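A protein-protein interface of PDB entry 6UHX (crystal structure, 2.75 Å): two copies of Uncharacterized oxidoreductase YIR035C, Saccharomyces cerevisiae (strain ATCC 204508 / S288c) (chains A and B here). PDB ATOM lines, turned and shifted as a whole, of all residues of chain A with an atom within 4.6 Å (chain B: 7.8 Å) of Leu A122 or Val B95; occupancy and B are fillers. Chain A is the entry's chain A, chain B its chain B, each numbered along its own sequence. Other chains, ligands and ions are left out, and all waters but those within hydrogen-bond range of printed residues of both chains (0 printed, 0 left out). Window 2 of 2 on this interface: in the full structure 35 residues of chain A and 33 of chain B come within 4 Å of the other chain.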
ATOM      1  N   VAL A 118       2.992   0.695   0.256  1.00  0.00           N
ATOM      2  CA  VAL A 118       4.366   0.998  -0.131  1.00  0.00           C
ATOM      3  C   VAL A 118       4.553   0.805  -1.630  1.00  0.00           C
ATOM      4  O   VAL A 118       5.170   1.639  -2.302  1.00  0.00           O
ATOM      5  CB  VAL A 118       5.352   0.141   0.684  1.00  0.00           C
ATOM      6  CG1 VAL A 118       6.776   0.398   0.226  1.00  0.00           C
ATOM      7  CG2 VAL A 118       5.209   0.442   2.168  1.00  0.00           C
ATOM      8  N   GLY A 119       4.011  -0.283  -2.182  1.00  0.00           N
ATOM      9  CA  GLY A 119       4.124  -0.535  -3.609  1.00  0.00           C
ATOM     10  C   GLY A 119       3.557   0.567  -4.480  1.00  0.00           C
ATOM     11  O   GLY A 119       3.983   0.718  -5.631  1.00  0.00           O
ATOM     12  N   ILE A 120       2.606   1.340  -3.962  1.00  0.00           N
ATOM     13  CA  ILE A 120       2.067   2.470  -4.708  1.00  0.00           C
ATOM     14  C   ILE A 120       2.908   3.730  -4.510  1.00  0.00           C
ATOM     15  O   ILE A 120       3.051   4.530  -5.441  1.00  0.00           O
ATOM     16  CB  ILE A 120       0.599   2.713  -4.309  1.00  0.00           C
ATOM     17  CG1 ILE A 120      -0.240   1.463  -4.582  1.00  0.00           C
ATOM     18  CG2 ILE A 120       0.020   3.907  -5.055  1.00  0.00           C
ATOM     19  CD1 ILE A 120      -1.652   1.544  -4.041  1.00  0.00           C
ATOM     20  N   ALA A 121       3.489   3.913  -3.327  1.00  0.00           N
ATOM     21  CA  ALA A 121       4.254   5.109  -3.004  1.00  0.00           C
ATOM     22  C   ALA A 121       5.761   4.912  -3.124  1.00  0.00           C
ATOM     23  O   ALA A 121       6.510   5.873  -2.927  1.00  0.00           O
ATOM     24  CB  ALA A 121       3.911   5.588  -1.589  1.00  0.00           C
ATOM     25  N   LEU A 122       6.222   3.703  -3.441  1.00  0.00           N
ATOM     26  CA  LEU A 122       7.653   3.439  -3.561  1.00  0.00           C
ATOM     27  C   LEU A 122       8.292   4.201  -4.724  1.00  0.00           C
ATOM     28  O   LEU A 122       9.394   4.737  -4.554  1.00  0.00           O
ATOM     29  CB  LEU A 122       7.919   1.938  -3.707  1.00  0.00           C
ATOM     30  CG  LEU A 122       9.378   1.503  -3.552  1.00  0.00           C
ATOM     31  CD1 LEU A 122       9.972   2.059  -2.268  1.00  0.00           C
ATOM     32  CD2 LEU A 122       9.494  -0.013  -3.583  1.00  0.00           C
ATOM     33  N   PRO A 123       7.670   4.265  -5.913  1.00  0.00           N
ATOM     34  CA  PRO A 123       8.279   5.073  -6.985  1.00  0.00           C
ATOM     35  C   PRO A 123       8.502   6.523  -6.596  1.00  0.00           C
ATOM     36  O   PRO A 123       9.515   7.118  -6.986  1.00  0.00           O
ATOM     37  CB  PRO A 123       7.271   4.941  -8.136  1.00  0.00           C
ATOM     38  CG  PRO A 123       6.622   3.635  -7.904  1.00  0.00           C
ATOM     39  CD  PRO A 123       6.506   3.508  -6.414  1.00  0.00           C
ATOM     40  N   GLU A 124       7.585   7.112  -5.827  1.00  0.00           N
ATOM     41  CA  GLU A 124       7.778   8.479  -5.363  1.00  0.00           C
ATOM     42  C   GLU A 124       8.748   8.550  -4.190  1.00  0.00           C
ATOM     43  O   GLU A 124       9.446   9.558  -4.029  1.00  0.00           O
ATOM     44  CB  GLU A 124       6.434   9.095  -4.973  1.00  0.00           C
ATOM     45  CG  GLU A 124       5.409   9.121  -6.096  1.00  0.00           C
ATOM     46  CD  GLU A 124       5.881   9.911  -7.299  1.00  0.00           C
ATOM     47  OE1 GLU A 124       5.832   9.370  -8.423  1.00  0.00           O
ATOM     48  OE2 GLU A 124       6.304  11.072  -7.121  1.00  0.00           O
ATOM     49  N   LEU A 125       8.807   7.498  -3.367  1.00  0.00           N
ATOM     50  CA  LEU A 125       9.747   7.481  -2.252  1.00  0.00           C
ATOM     51  C   LEU A 125      11.187   7.347  -2.731  1.00  0.00           C
ATOM     52  O   LEU A 125      12.105   7.860  -2.082  1.00  0.00           O
ATOM     53  CB  LEU A 125       9.405   6.341  -1.292  1.00  0.00           C
ATOM     54  CG  LEU A 125       8.275   6.587  -0.289  1.00  0.00           C
ATOM     55  CD1 LEU A 125       7.761   5.271   0.276  1.00  0.00           C
ATOM     56  CD2 LEU A 125       8.740   7.503   0.829  1.00  0.00           C
ATOM     57  N   LYS A 126      11.403   6.662  -3.857  1.00  0.00           N
ATOM     58  CA  LYS A 126      12.756   6.510  -4.380  1.00  0.00           C
ATOM     59  C   LYS A 126      13.271   7.805  -4.994  1.00  0.00           C
ATOM     60  O   LYS A 126      14.484   8.040  -5.014  1.00  0.00           O
ATOM     61  CB  LYS A 126      12.797   5.382  -5.411  1.00  0.00           C
ATOM     62  CG  LYS A 126      12.586   3.994  -4.825  1.00  0.00           C
ATOM     63  CD  LYS A 126      12.268   2.980  -5.914  1.00  0.00           C
ATOM     64  CE  LYS A 126      13.307   3.019  -7.023  1.00  0.00           C
ATOM     65  NZ  LYS A 126      12.994   2.056  -8.115  1.00  0.00           N
ATOM     66  N   LEU A 164      12.374  -4.849   2.591  1.00  0.00           N
ATOM     67  CA  LEU A 164      12.340  -3.590   1.854  1.00  0.00           C
ATOM     68  C   LEU A 164      13.661  -2.839   1.978  1.00  0.00           C
ATOM     69  O   LEU A 164      14.125  -2.221   1.012  1.00  0.00           O
ATOM     70  CB  LEU A 164      11.181  -2.725   2.349  1.00  0.00           C
ATOM     71  CG  LEU A 164      11.036  -1.335   1.726  1.00  0.00           C
ATOM     72  CD1 LEU A 164      10.852  -1.439   0.220  1.00  0.00           C
ATOM     73  CD2 LEU A 164       9.876  -0.584   2.360  1.00  0.00           C
ATOM     74  N   GLU A 167      16.190  -4.839  -0.222  1.00  0.00           N
ATOM     75  CA  GLU A 167      15.914  -4.942  -1.650  1.00  0.00           C
ATOM     76  C   GLU A 167      16.213  -3.630  -2.366  1.00  0.00           C
ATOM     77  O   GLU A 167      17.087  -3.569  -3.237  1.00  0.00           O
ATOM     78  CB  GLU A 167      14.460  -5.358  -1.872  1.00  0.00           C
ATOM     79  CG  GLU A 167      14.161  -5.853  -3.272  1.00  0.00           C
ATOM     80  CD  GLU A 167      13.325  -7.114  -3.270  1.00  0.00           C
ATOM     81  OE1 GLU A 167      13.516  -7.955  -2.366  1.00  0.00           O
ATOM     82  OE2 GLU A 167      12.470  -7.261  -4.165  1.00  0.00           O
ATOM     83  N   GLU A 168      15.491  -2.572  -2.013  1.00  0.00           N
ATOM     84  CA  GLU A 168      15.663  -1.248  -2.608  1.00  0.00           C
ATOM     85  C   GLU A 168      16.362  -0.364  -1.578  1.00  0.00           C
ATOM     86  O   GLU A 168      15.721   0.239  -0.715  1.00  0.00           O
ATOM     87  CB  GLU A 168      14.323  -0.659  -3.041  1.00  0.00           C
ATOM     88  CG  GLU A 168      14.439   0.601  -3.884  1.00  0.00           C
ATOM     89  CD  GLU A 168      15.159   0.366  -5.200  1.00  0.00           C
ATOM     90  OE1 GLU A 168      16.403   0.461  -5.228  1.00  0.00           O
ATOM     91  OE2 GLU A 168      14.477   0.083  -6.207  1.00  0.00           O
ATOM     92  N   VAL A 171      15.645   3.695  -0.743  1.00  0.00           N
ATOM     93  CA  VAL A 171      14.872   4.058   0.427  1.00  0.00           C
ATOM     94  C   VAL A 171      15.386   3.250   1.610  1.00  0.00           C
ATOM     95  O   VAL A 171      16.084   2.243   1.458  1.00  0.00           O
ATOM     96  CB  VAL A 171      13.361   3.828   0.209  1.00  0.00           C
ATOM     97  CG1 VAL A 171      12.888   4.556  -1.038  1.00  0.00           C
ATOM     98  CG2 VAL A 171      13.062   2.338   0.104  1.00  0.00           C
ATOM     99  N   GLN B  93       8.978 -11.857  -6.439  1.00  0.00           N
ATOM    100  CA  GLN B  93       8.913 -10.604  -7.177  1.00  0.00           C
ATOM    101  C   GLN B  93       9.612  -9.514  -6.378  1.00  0.00           C
ATOM    102  O   GLN B  93       9.913  -9.676  -5.192  1.00  0.00           O
ATOM    103  CB  GLN B  93       7.462 -10.215  -7.479  1.00  0.00           C
ATOM    104  CG  GLN B  93       6.569 -10.164  -6.250  1.00  0.00           C
ATOM    105  CD  GLN B  93       5.097 -10.080  -6.601  1.00  0.00           C
ATOM    106  OE1 GLN B  93       4.257  -9.803  -5.744  1.00  0.00           O
ATOM    107  NE2 GLN B  93       4.776 -10.320  -7.868  1.00  0.00           N
ATOM    108  N   ASN B  94       9.860  -8.392  -7.048  1.00  0.00           N
ATOM    109  CA  ASN B  94      10.525  -7.256  -6.433  1.00  0.00           C
ATOM    110  C   ASN B  94       9.521  -6.392  -5.673  1.00  0.00           C
ATOM    111  O   ASN B  94       8.307  -6.472  -5.880  1.00  0.00           O
ATOM    112  CB  ASN B  94      11.248  -6.420  -7.491  1.00  0.00           C
ATOM    113  CG  ASN B  94      12.190  -5.397  -6.885  1.00  0.00           C
ATOM    114  OD1 ASN B  94      11.804  -4.253  -6.636  1.00  0.00           O
ATOM    115  ND2 ASN B  94      13.429  -5.804  -6.639  1.00  0.00           N
ATOM    116  N   VAL B  95      10.049  -5.558  -4.771  1.00  0.00           N
ATOM    117  CA  VAL B  95       9.201  -4.638  -4.021  1.00  0.00           C
ATOM    118  C   VAL B  95       8.542  -3.632  -4.954  1.00  0.00           C
ATOM    119  O   VAL B  95       7.437  -3.148  -4.678  1.00  0.00           O
ATOM    120  CB  VAL B  95      10.014  -3.936  -2.916  1.00  0.00           C
ATOM    121  CG1 VAL B  95      10.143  -4.838  -1.699  1.00  0.00           C
ATOM    122  CG2 VAL B  95      11.383  -3.530  -3.438  1.00  0.00           C
ATOM    123  N   ASN B  96       9.197  -3.302  -6.066  1.00  0.00           N
ATOM    124  CA  ASN B  96       8.620  -2.411  -7.062  1.00  0.00           C
ATOM    125  C   ASN B  96       7.624  -3.113  -7.978  1.00  0.00           C
ATOM    126  O   ASN B  96       7.001  -2.450  -8.815  1.00  0.00           O
ATOM    127  CB  ASN B  96       9.728  -1.769  -7.903  1.00  0.00           C
ATOM    128  CG  ASN B  96      10.477  -0.684  -7.152  1.00  0.00           C
ATOM    129  OD1 ASN B  96      11.447  -0.958  -6.445  1.00  0.00           O
ATOM    130  ND2 ASN B  96      10.030   0.557  -7.304  1.00  0.00           N
ATOM    131  N   GLU B  97       7.464  -4.430  -7.844  1.00  0.00           N
ATOM    132  CA  GLU B  97       6.538  -5.213  -8.661  1.00  0.00           C
ATOM    133  C   GLU B  97       5.751  -6.164  -7.757  1.00  0.00           C
ATOM    134  O   GLU B  97       5.783  -7.385  -7.914  1.00  0.00           O
ATOM    135  CB  GLU B  97       7.280  -5.987  -9.749  1.00  0.00           C
ATOM    136  CG  GLU B  97       8.112  -5.121 -10.681  1.00  0.00           C
ATOM    137  CD  GLU B  97       7.479  -4.960 -12.048  1.00  0.00           C
ATOM    138  OE1 GLU B  97       7.156  -5.988 -12.679  1.00  0.00           O
ATOM    139  OE2 GLU B  97       7.302  -3.805 -12.488  1.00  0.00           O
ATOM    140  N   ILE B  98       5.026  -5.591  -6.800  1.00  0.00           N
ATOM    141  CA  ILE B  98       4.307  -6.353  -5.786  1.00  0.00           C
ATOM    142  C   ILE B  98       2.861  -6.528  -6.226  1.00  0.00           C
ATOM    143  O   ILE B  98       2.195  -5.556  -6.604  1.00  0.00           O
ATOM    144  CB  ILE B  98       4.383  -5.661  -4.414  1.00  0.00           C
ATOM    145  CG1 ILE B  98       5.751  -5.891  -3.772  1.00  0.00           C
ATOM    146  CG2 ILE B  98       3.271  -6.156  -3.497  1.00  0.00           C
ATOM    147  CD1 ILE B  98       5.871  -5.320  -2.375  1.00  0.00           C
ATOM    148  N   ASP B  99       2.377  -7.768  -6.182  1.00  0.00           N
ATOM    149  CA  ASP B  99       0.973  -8.090  -6.417  1.00  0.00           C
ATOM    150  C   ASP B  99       0.382  -8.558  -5.092  1.00  0.00           C
ATOM    151  O   ASP B  99       0.757  -9.617  -4.578  1.00  0.00           O
ATOM    152  CB  ASP B  99       0.825  -9.157  -7.501  1.00  0.00           C
ATOM    153  CG  ASP B  99      -0.603  -9.287  -8.002  1.00  0.00           C
ATOM    154  OD1 ASP B  99      -1.484  -8.560  -7.497  1.00  0.00           O
ATOM    155  OD2 ASP B  99      -0.842 -10.118  -8.903  1.00  0.00           O
ATOM    156  N   TRP B 103       0.142 -12.132  -3.192  1.00  0.00           N
ATOM    157  CA  TRP B 103       0.763 -12.306  -1.884  1.00  0.00           C
ATOM    158  C   TRP B 103      -0.183 -12.981  -0.900  1.00  0.00           C
ATOM    159  O   TRP B 103       0.265 -13.741  -0.033  1.00  0.00           O
ATOM    160  CB  TRP B 103       1.217 -10.954  -1.330  1.00  0.00           C
ATOM    161  CG  TRP B 103       2.622 -10.582  -1.695  1.00  0.00           C
ATOM    162  CD1 TRP B 103       3.214 -10.715  -2.917  1.00  0.00           C
ATOM    163  CD2 TRP B 103       3.613 -10.012  -0.830  1.00  0.00           C
ATOM    164  NE1 TRP B 103       4.512 -10.264  -2.867  1.00  0.00           N
ATOM    165  CE2 TRP B 103       4.781  -9.827  -1.595  1.00  0.00           C
ATOM    166  CE3 TRP B 103       3.625  -9.641   0.519  1.00  0.00           C
ATOM    167  CZ2 TRP B 103       5.949  -9.289  -1.059  1.00  0.00           C
ATOM    168  CZ3 TRP B 103       4.786  -9.106   1.050  1.00  0.00           C
ATOM    169  CH2 TRP B 103       5.931  -8.935   0.262  1.00  0.00           C
ATOM    170  N   TYR B 143      17.711 -12.641   5.070  1.00  0.00           N
ATOM    171  CA  TYR B 143      17.130 -11.994   3.902  1.00  0.00           C
ATOM    172  C   TYR B 143      17.402 -12.813   2.649  1.00  0.00           C
ATOM    173  O   TYR B 143      18.512 -13.312   2.444  1.00  0.00           O
ATOM    174  CB  TYR B 143      17.687 -10.580   3.723  1.00  0.00           C
ATOM    175  CG  TYR B 143      17.418  -9.997   2.352  1.00  0.00           C
ATOM    176  CD1 TYR B 143      16.133  -9.626   1.976  1.00  0.00           C
ATOM    177  CD2 TYR B 143      18.444  -9.826   1.431  1.00  0.00           C
ATOM    178  CE1 TYR B 143      15.878  -9.097   0.725  1.00  0.00           C
ATOM    179  CE2 TYR B 143      18.199  -9.299   0.176  1.00  0.00           C
ATOM    180  CZ  TYR B 143      16.914  -8.936  -0.171  1.00  0.00           C
ATOM    181  OH  TYR B 143      16.663  -8.410  -1.417  1.00  0.00           O
ATOM    182  N   SER B 146      13.960 -11.007  -3.331  1.00  0.00           N
ATOM    183  CA  SER B 146      12.635 -11.142  -3.935  1.00  0.00           C
ATOM    184  C   SER B 146      11.774 -12.213  -3.270  1.00  0.00           C
ATOM    185  O   SER B 146      10.700 -12.545  -3.787  1.00  0.00           O
ATOM    186  CB  SER B 146      12.733 -11.413  -5.443  1.00  0.00           C
ATOM    187  OG  SER B 146      13.419 -10.361  -6.098  1.00  0.00           O
ATOM    188  N   GLY B 148       9.774 -11.958  -0.867  1.00  0.00           N
ATOM    189  CA  GLY B 148       8.970 -11.102  -0.017  1.00  0.00           C
ATOM    190  C   GLY B 148       7.837 -11.810   0.693  1.00  0.00           C
ATOM    191  O   GLY B 148       7.772 -11.806   1.926  1.00  0.00           O
ATOM    192  N   SER B 197      13.065 -12.785 -10.972  1.00  0.00           N
ATOM    193  CA  SER B 197      12.830 -11.789  -9.939  1.00  0.00           C
ATOM    194  C   SER B 197      13.978 -11.636  -8.955  1.00  0.00           C
ATOM    195  O   SER B 197      14.068 -10.594  -8.300  1.00  0.00           O
ATOM    196  CB  SER B 197      11.557 -12.132  -9.154  1.00  0.00           C
ATOM    197  OG  SER B 197      10.580 -12.715  -9.999  1.00  0.00           O
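The side-chain hydroxyl (OH) of Tyr B143 sits at hydrogen-bond distance from the side-chain carboxylate (OE1) of Glu A167 (3.3 Å). The side-chain amide oxygen (OD1) of Asn B96 sits close to the side-chain carboxylate (OE2) of Glu A168 (3.2 Å). The side-chain carboxylate (OE1) of Glu A167 is in hydrogen-bond range of the backbone NH (N) of Ser B146. The side-chain amino group (NZ) of Lys A126 lies close to the side-chain amide nitrogen (ND2) of Asn B96 (3.4 Å). ND2 of Asn B94 lies close to OE2 of Glu A167 (3.0 Å). The backbone NH (N) of Val B95 lies within hydrogen-bond range of the side-chain carboxylate (OE2) of Glu A167, at 3.0 Å.
The side-chain amide oxygen (OD1) of Asn B94 lies within hydrogen-bond range of the backbone NH (N) of Asn B96 (2.8 Å). The backbone NH of Gln B93 is in hydrogen-bond range of the backbone carbonyl oxygen of Ser B146, at 3.2 Å. The backbone NH (N) of Asp B99 lies within hydrogen-bond range of the side-chain amide oxygen (OE1) of Gln B93 (2.8 Å). The side-chain amino group (NZ) of Lys A126 lies within salt-bridge range of the side-chain carboxylate (OE2) of Glu A168 (3.1 Å). OE1 of Gln B93 sits at hydrogen-bond distance from NE1 of Trp B103. NE2 of Gln B93 sits close to O of Glu B97, 3.1 Å away.
Among the printed residues, pairs that only touch across the chains: Leu A122 with Asn B96 (3.6 Å), Glu A167 with Gln B93 (3.7 Å), Leu A122 with Val B95 (3.9 Å) and Leu A164 with Val B95 (3.97 Å).
No residue of chain B comes within 4 Å of Ala A121. Leu A122 touches just these residues of chain B: Val B95 (3.9 Å) and Asn B96 (3.6 Å). Of the printed residues of chain B, Glu A168 touches Asn B96. Of the printed residues of chain A, Val B95 touches Leu A122 (3.9 Å), Leu A164 (3.97 Å) and Glu A167 (3.0 Å). Printed residues of chain A within 4 Å of Asn B96: Leu A122, Lys A126 and Glu A168. Glu B97 touches none of the printed residues of chain A. Gly B148 touches none of the printed residues of chain A. The nearest printed residue of chain B that does not touch Glu A167 is Asn B96 (5.5 Å).
Printed residues of chain B that touch a printed residue of chain A: Gln B93, Asn B94, Val B95, Asn B96, Tyr B143 and Ser B146. Hydrophobic or aromatic side chains of chain B that line the printed part of chain A: Val B95 and Tyr B143. Of the 13 printed residues of chain A, 5 touch a printed residue of chain B. Among the printed residues, no Asp or Glu carboxylate lies within 4 Å of a Lys or Arg side-chain nitrogen of the other chain.
No position is printed for both chains.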
